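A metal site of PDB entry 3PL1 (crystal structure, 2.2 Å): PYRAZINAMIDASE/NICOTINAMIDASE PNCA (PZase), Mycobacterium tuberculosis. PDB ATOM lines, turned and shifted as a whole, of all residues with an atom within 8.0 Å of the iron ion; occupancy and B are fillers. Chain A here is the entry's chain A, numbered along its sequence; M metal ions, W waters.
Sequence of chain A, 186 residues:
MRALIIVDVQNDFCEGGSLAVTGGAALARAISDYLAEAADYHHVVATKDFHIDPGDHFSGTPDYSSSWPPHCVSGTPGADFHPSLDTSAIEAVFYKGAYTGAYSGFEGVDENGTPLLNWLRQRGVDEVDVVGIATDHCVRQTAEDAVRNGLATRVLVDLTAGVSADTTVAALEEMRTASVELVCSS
The side-chain carboxylate of Asp 49 is in salt-bridge range of the side-chain amino group of Lys 96 (3.3 Å). A ring nitrogen (ND1) of His 71 lies within hydrogen-bond range of the backbone carbonyl oxygen of Pro 69, at 2.8 Å. N of His 51 sits at hydrogen-bond distance from O of Cys 72 (2.9 Å). The backbone carbonyl oxygen (O) of Gly 97 is in hydrogen-bond range of a ring nitrogen (ND1) of His 51, at 2.5 Å. The backbone carbonyl oxygen (O) of His 57 lies within hydrogen-bond range of the backbone NH (N) of Trp 68, at 3.0 Å.
Within 4 Å of the iron ion: Asp 49, His 51, His 57 and His 71. Along chain A the residues within 4 Å of the iron ion span positions 49 to 71. The nearest printed residue that does not touch the iron ion is Ala 102 (4.9 Å).
The iron ion is bound by OD2 of Asp 49, NE2 of His 71, water W2, NE2 of His 51 and NE2 of His 57. The iron ion has five donor atoms within binding distance.
Water W2 lies within hydrogen-bond range of the side-chain carboxylate (OD1) of Asp 49 and the backbone NH (N) of Ala 102.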
ATOM      1  N   ASP A   8       8.567  -5.597   5.363  1.00  0.00           N
ATOM      2  CA  ASP A   8       9.762  -5.462   6.193  1.00  0.00           C
ATOM      3  C   ASP A   8       9.986  -6.549   7.248  1.00  0.00           C
ATOM      4  O   ASP A   8      10.357  -6.283   8.353  1.00  0.00           O
ATOM      5  CB  ASP A   8       9.797  -4.090   6.841  1.00  0.00           C
ATOM      6  CG  ASP A   8       9.960  -2.925   5.842  1.00  0.00           C
ATOM      7  OD1 ASP A   8       9.851  -3.030   4.588  1.00  0.00           O
ATOM      8  OD2 ASP A   8      10.254  -1.836   6.342  1.00  0.00           O
ATOM      9  N   PHE A  13      14.567  -5.974  12.336  1.00  0.00           N
ATOM     10  CA  PHE A  13      13.271  -5.685  12.946  1.00  0.00           C
ATOM     11  C   PHE A  13      12.739  -6.861  13.818  1.00  0.00           C
ATOM     12  O   PHE A  13      11.646  -6.768  14.366  1.00  0.00           O
ATOM     13  CB  PHE A  13      12.223  -5.309  11.838  1.00  0.00           C
ATOM     14  CG  PHE A  13      12.608  -4.124  10.966  1.00  0.00           C
ATOM     15  CD1 PHE A  13      13.071  -2.929  11.539  1.00  0.00           C
ATOM     16  CD2 PHE A  13      12.516  -4.189   9.598  1.00  0.00           C
ATOM     17  CE1 PHE A  13      13.453  -1.812  10.705  1.00  0.00           C
ATOM     18  CE2 PHE A  13      12.908  -3.072   8.754  1.00  0.00           C
ATOM     19  CZ  PHE A  13      13.333  -1.878   9.330  1.00  0.00           C
ATOM     20  N   LEU A  19      16.919  -2.901  15.434  1.00  0.00           N
ATOM     21  CA  LEU A  19      15.600  -2.299  15.724  1.00  0.00           C
ATOM     22  C   LEU A  19      14.535  -3.376  16.094  1.00  0.00           C
ATOM     23  O   LEU A  19      13.385  -3.362  15.564  1.00  0.00           O
ATOM     24  CB  LEU A  19      15.176  -1.482  14.505  1.00  0.00           C
ATOM     25  CG  LEU A  19      15.214   0.044  14.574  1.00  0.00           C
ATOM     26  CD1 LEU A  19      15.704   0.654  15.893  1.00  0.00           C
ATOM     27  CD2 LEU A  19      15.853   0.765  13.420  1.00  0.00           C
ATOM     28  N   LYS A  48      11.301  -4.455   1.407  1.00  0.00           N
ATOM     29  CA  LYS A  48      12.437  -4.487   2.320  1.00  0.00           C
ATOM     30  C   LYS A  48      12.964  -3.067   2.458  1.00  0.00           C
ATOM     31  O   LYS A  48      13.183  -2.433   1.439  1.00  0.00           O
ATOM     32  CB  LYS A  48      13.617  -5.302   1.674  1.00  0.00           C
ATOM     33  CG  LYS A  48      13.540  -6.838   1.717  1.00  0.00           C
ATOM     34  CD  LYS A  48      14.925  -7.468   1.404  1.00  0.00           C
ATOM     35  CE  LYS A  48      15.025  -8.891   2.006  1.00  0.00           C
ATOM     36  NZ  LYS A  48      16.189  -9.607   1.436  1.00  0.00           N
ATOM     37  N   ASP A  49      13.223  -2.603   3.691  1.00  0.00           N
ATOM     38  CA  ASP A  49      14.099  -1.451   3.929  1.00  0.00           C
ATOM     39  C   ASP A  49      15.552  -1.840   3.493  1.00  0.00           C
ATOM     40  O   ASP A  49      16.050  -2.953   3.772  1.00  0.00           O
ATOM     41  CB  ASP A  49      14.071  -1.159   5.425  1.00  0.00           C
ATOM     42  CG  ASP A  49      14.055   0.358   5.755  1.00  0.00           C
ATOM     43  OD1 ASP A  49      13.699   1.123   4.841  1.00  0.00           O
ATOM     44  OD2 ASP A  49      14.405   0.781   6.930  1.00  0.00           O
ATOM     45  N   PHE A  50      16.244  -0.967   2.768  1.00  0.00           N
ATOM     46  CA  PHE A  50      17.542  -1.388   2.181  1.00  0.00           C
ATOM     47  C   PHE A  50      18.427  -0.155   1.949  1.00  0.00           C
ATOM     48  O   PHE A  50      18.261   0.574   0.937  1.00  0.00           O
ATOM     49  CB  PHE A  50      17.313  -2.158   0.880  1.00  0.00           C
ATOM     50  CG  PHE A  50      18.519  -2.891   0.373  1.00  0.00           C
ATOM     51  CD1 PHE A  50      18.853  -4.152   0.870  1.00  0.00           C
ATOM     52  CD2 PHE A  50      19.300  -2.334  -0.654  1.00  0.00           C
ATOM     53  CE1 PHE A  50      19.991  -4.902   0.343  1.00  0.00           C
ATOM     54  CE2 PHE A  50      20.417  -3.032  -1.162  1.00  0.00           C
ATOM     55  CZ  PHE A  50      20.771  -4.350  -0.654  1.00  0.00           C
ATOM     56  N   HIS A  51      19.336   0.083   2.900  1.00  0.00           N
ATOM     57  CA  HIS A  51      20.070   1.313   2.960  1.00  0.00           C
ATOM     58  C   HIS A  51      21.529   1.149   2.497  1.00  0.00           C
ATOM     59  O   HIS A  51      22.273   0.296   3.039  1.00  0.00           O
ATOM     60  CB  HIS A  51      20.031   1.812   4.412  1.00  0.00           C
ATOM     61  CG  HIS A  51      18.661   2.265   4.812  1.00  0.00           C
ATOM     62  ND1 HIS A  51      17.920   3.132   4.028  1.00  0.00           N
ATOM     63  CD2 HIS A  51      17.914   2.021   5.934  1.00  0.00           C
ATOM     64  CE1 HIS A  51      16.771   3.375   4.639  1.00  0.00           C
ATOM     65  NE2 HIS A  51      16.762   2.745   5.795  1.00  0.00           N
ATOM     66  N   PRO A  54      21.831   6.499   3.374  1.00  0.00           N
ATOM     67  CA  PRO A  54      20.650   7.326   3.662  1.00  0.00           C
ATOM     68  C   PRO A  54      20.993   8.571   4.549  1.00  0.00           C
ATOM     69  O   PRO A  54      20.084   9.184   5.079  1.00  0.00           O
ATOM     70  CB  PRO A  54      19.793   6.367   4.430  1.00  0.00           C
ATOM     71  CG  PRO A  54      20.819   5.647   5.315  1.00  0.00           C
ATOM     72  CD  PRO A  54      22.049   5.470   4.421  1.00  0.00           C
ATOM     73  N   HIS A  57      19.126   9.878   8.134  1.00  0.00           N
ATOM     74  CA  HIS A  57      18.289   8.776   8.578  1.00  0.00           C
ATOM     75  C   HIS A  57      18.928   7.889   9.694  1.00  0.00           C
ATOM     76  O   HIS A  57      18.195   7.231  10.477  1.00  0.00           O
ATOM     77  CB  HIS A  57      17.913   7.907   7.359  1.00  0.00           C
ATOM     78  CG  HIS A  57      16.918   6.807   7.639  1.00  0.00           C
ATOM     79  ND1 HIS A  57      15.615   7.041   8.018  1.00  0.00           N
ATOM     80  CD2 HIS A  57      17.050   5.462   7.561  1.00  0.00           C
ATOM     81  CE1 HIS A  57      14.976   5.889   8.158  1.00  0.00           C
ATOM     82  NE2 HIS A  57      15.821   4.904   7.890  1.00  0.00           N
ATOM     83  N   PHE A  58      20.254   7.835   9.714  1.00  0.00           N
ATOM     84  CA  PHE A  58      21.051   7.103  10.708  1.00  0.00           C
ATOM     85  C   PHE A  58      21.735   8.141  11.542  1.00  0.00           C
ATOM     86  O   PHE A  58      22.147   9.153  11.015  1.00  0.00           O
ATOM     87  CB  PHE A  58      22.225   6.328  10.056  1.00  0.00           C
ATOM     88  CG  PHE A  58      21.796   5.148   9.263  1.00  0.00           C
ATOM     89  CD1 PHE A  58      20.487   4.666   9.305  1.00  0.00           C
ATOM     90  CD2 PHE A  58      22.733   4.485   8.457  1.00  0.00           C
ATOM     91  CE1 PHE A  58      20.095   3.539   8.560  1.00  0.00           C
ATOM     92  CE2 PHE A  58      22.365   3.340   7.706  1.00  0.00           C
ATOM     93  CZ  PHE A  58      21.030   2.847   7.762  1.00  0.00           C
ATOM     94  N   TRP A  68      17.699   7.101  13.416  1.00  0.00           N
ATOM     95  CA  TRP A  68      17.687   5.709  13.870  1.00  0.00           C
ATOM     96  C   TRP A  68      19.100   5.109  14.045  1.00  0.00           C
ATOM     97  O   TRP A  68      20.021   5.563  13.408  1.00  0.00           O
ATOM     98  CB  TRP A  68      16.898   4.922  12.855  1.00  0.00           C
ATOM     99  CG  TRP A  68      15.509   5.521  12.623  1.00  0.00           C
ATOM    100  CD1 TRP A  68      15.118   6.412  11.642  1.00  0.00           C
ATOM    101  CD2 TRP A  68      14.327   5.218  13.366  1.00  0.00           C
ATOM    102  NE1 TRP A  68      13.771   6.699  11.762  1.00  0.00           N
ATOM    103  CE2 TRP A  68      13.268   6.000  12.823  1.00  0.00           C
ATOM    104  CE3 TRP A  68      14.079   4.377  14.469  1.00  0.00           C
ATOM    105  CZ2 TRP A  68      11.959   5.934  13.311  1.00  0.00           C
ATOM    106  CZ3 TRP A  68      12.790   4.346  14.987  1.00  0.00           C
ATOM    107  CH2 TRP A  68      11.729   5.116  14.401  1.00  0.00           C
ATOM    108  N   PRO A  69      19.265   4.054  14.866  1.00  0.00           N
ATOM    109  CA  PRO A  69      20.584   3.385  14.730  1.00  0.00           C
ATOM    110  C   PRO A  69      20.649   2.696  13.325  1.00  0.00           C
ATOM    111  O   PRO A  69      19.586   2.398  12.735  1.00  0.00           O
ATOM    112  CB  PRO A  69      20.608   2.332  15.841  1.00  0.00           C
ATOM    113  CG  PRO A  69      19.034   2.013  16.055  1.00  0.00           C
ATOM    114  CD  PRO A  69      18.340   3.344  15.785  1.00  0.00           C
ATOM    115  N   PRO A  70      21.874   2.512  12.783  1.00  0.00           N
ATOM    116  CA  PRO A  70      22.009   1.837  11.491  1.00  0.00           C
ATOM    117  C   PRO A  70      21.202   0.514  11.429  1.00  0.00           C
ATOM    118  O   PRO A  70      21.285  -0.315  12.375  1.00  0.00           O
ATOM    119  CB  PRO A  70      23.497   1.529  11.417  1.00  0.00           C
ATOM    120  CG  PRO A  70      24.103   2.727  12.159  1.00  0.00           C
ATOM    121  CD  PRO A  70      23.183   2.945  13.332  1.00  0.00           C
ATOM    122  N   HIS A  71      20.499   0.269  10.325  1.00  0.00           N
ATOM    123  CA  HIS A  71      19.696  -0.944  10.245  1.00  0.00           C
ATOM    124  C   HIS A  71      19.556  -1.266   8.747  1.00  0.00           C
ATOM    125  O   HIS A  71      19.640  -0.342   7.932  1.00  0.00           O
ATOM    126  CB  HIS A  71      18.263  -0.755  10.876  1.00  0.00           C
ATOM    127  CG  HIS A  71      17.511   0.416  10.323  1.00  0.00           C
ATOM    128  ND1 HIS A  71      17.794   1.734  10.699  1.00  0.00           N
ATOM    129  CD2 HIS A  71      16.531   0.483   9.378  1.00  0.00           C
ATOM    130  CE1 HIS A  71      17.018   2.562  10.012  1.00  0.00           C
ATOM    131  NE2 HIS A  71      16.245   1.841   9.195  1.00  0.00           N
ATOM    132  N   CYS A  72      19.360  -2.554   8.400  1.00  0.00           N
ATOM    133  CA  CYS A  72      19.066  -2.968   7.030  1.00  0.00           C
ATOM    134  C   CYS A  72      20.092  -2.374   6.022  1.00  0.00           C
ATOM    135  O   CYS A  72      19.745  -1.883   4.956  1.00  0.00           O
ATOM    136  CB  CYS A  72      17.604  -2.579   6.652  1.00  0.00           C
ATOM    137  SG  CYS A  72      16.368  -3.224   7.779  1.00  0.00           S
ATOM    138  N   LYS A  96      13.408  -0.164  -0.787  1.00  0.00           N
ATOM    139  CA  LYS A  96      13.262   1.309  -0.643  1.00  0.00           C
ATOM    140  C   LYS A  96      14.359   1.787   0.337  1.00  0.00           C
ATOM    141  O   LYS A  96      14.808   1.010   1.185  1.00  0.00           O
ATOM    142  CB  LYS A  96      11.878   1.638  -0.012  1.00  0.00           C
ATOM    143  CG  LYS A  96      11.727   0.847   1.313  1.00  0.00           C
ATOM    144  CD  LYS A  96      10.384   1.015   2.039  1.00  0.00           C
ATOM    145  CE  LYS A  96      10.097  -0.157   3.032  1.00  0.00           C
ATOM    146  NZ  LYS A  96      10.498   0.338   4.360  1.00  0.00           N
ATOM    147  N   GLY A  97      14.731   3.058   0.247  1.00  0.00           N
ATOM    148  CA  GLY A  97      15.658   3.713   1.172  1.00  0.00           C
ATOM    149  C   GLY A  97      17.169   3.625   0.782  1.00  0.00           C
ATOM    150  O   GLY A  97      18.040   3.914   1.632  1.00  0.00           O
ATOM    151  N   THR A 100      18.135   7.268   1.097  1.00  0.00           N
ATOM    152  CA  THR A 100      17.193   8.120   1.785  1.00  0.00           C
ATOM    153  C   THR A 100      16.413   7.338   2.866  1.00  0.00           C
ATOM    154  O   THR A 100      16.250   6.135   2.736  1.00  0.00           O
ATOM    155  CB  THR A 100      16.213   8.762   0.715  1.00  0.00           C
ATOM    156  OG1 THR A 100      15.793  10.059   1.156  1.00  0.00           O
ATOM    157  CG2 THR A 100      14.987   7.819   0.357  1.00  0.00           C
ATOM    158  N   GLY A 101      15.988   8.003   3.938  1.00  0.00           N
ATOM    159  CA  GLY A 101      14.999   7.391   4.843  1.00  0.00           C
ATOM    160  C   GLY A 101      13.682   7.095   4.111  1.00  0.00           C
ATOM    161  O   GLY A 101      13.134   7.976   3.425  1.00  0.00           O
ATOM    162  N   ALA A 102      13.167   5.863   4.207  1.00  0.00           N
ATOM    163  CA  ALA A 102      11.876   5.521   3.543  1.00  0.00           C
ATOM    164  C   ALA A 102      10.733   5.210   4.561  1.00  0.00           C
ATOM    165  O   ALA A 102      10.966   4.562   5.621  1.00  0.00           O
ATOM    166  CB  ALA A 102      12.065   4.382   2.515  1.00  0.00           C
ATOM    167  N   TYR A 103       9.510   5.647   4.218  1.00  0.00           N
ATOM    168  CA  TYR A 103       8.342   5.484   5.116  1.00  0.00           C
ATOM    169  C   TYR A 103       7.303   4.438   4.699  1.00  0.00           C
ATOM    170  O   TYR A 103       6.646   3.926   5.548  1.00  0.00           O
ATOM    171  CB  TYR A 103       7.662   6.859   5.461  1.00  0.00           C
ATOM    172  CG  TYR A 103       8.693   7.848   5.932  1.00  0.00           C
ATOM    173  CD1 TYR A 103       9.259   7.743   7.221  1.00  0.00           C
ATOM    174  CD2 TYR A 103       9.177   8.844   5.053  1.00  0.00           C
ATOM    175  CE1 TYR A 103      10.270   8.644   7.611  1.00  0.00           C
ATOM    176  CE2 TYR A 103      10.177   9.757   5.431  1.00  0.00           C
ATOM    177  CZ  TYR A 103      10.729   9.651   6.716  1.00  0.00           C
ATOM    178  OH  TYR A 103      11.735  10.541   7.100  1.00  0.00           O
HETATM  179 FE    FE M   1      15.168   2.722   7.453  1.00  0.00          FE
HETATM  180  O   HOH W   1      12.475   3.639   7.883  1.00  0.00           O
HETATM  181  O   HOH W   2      13.812   3.487   5.818  1.00  0.00           O
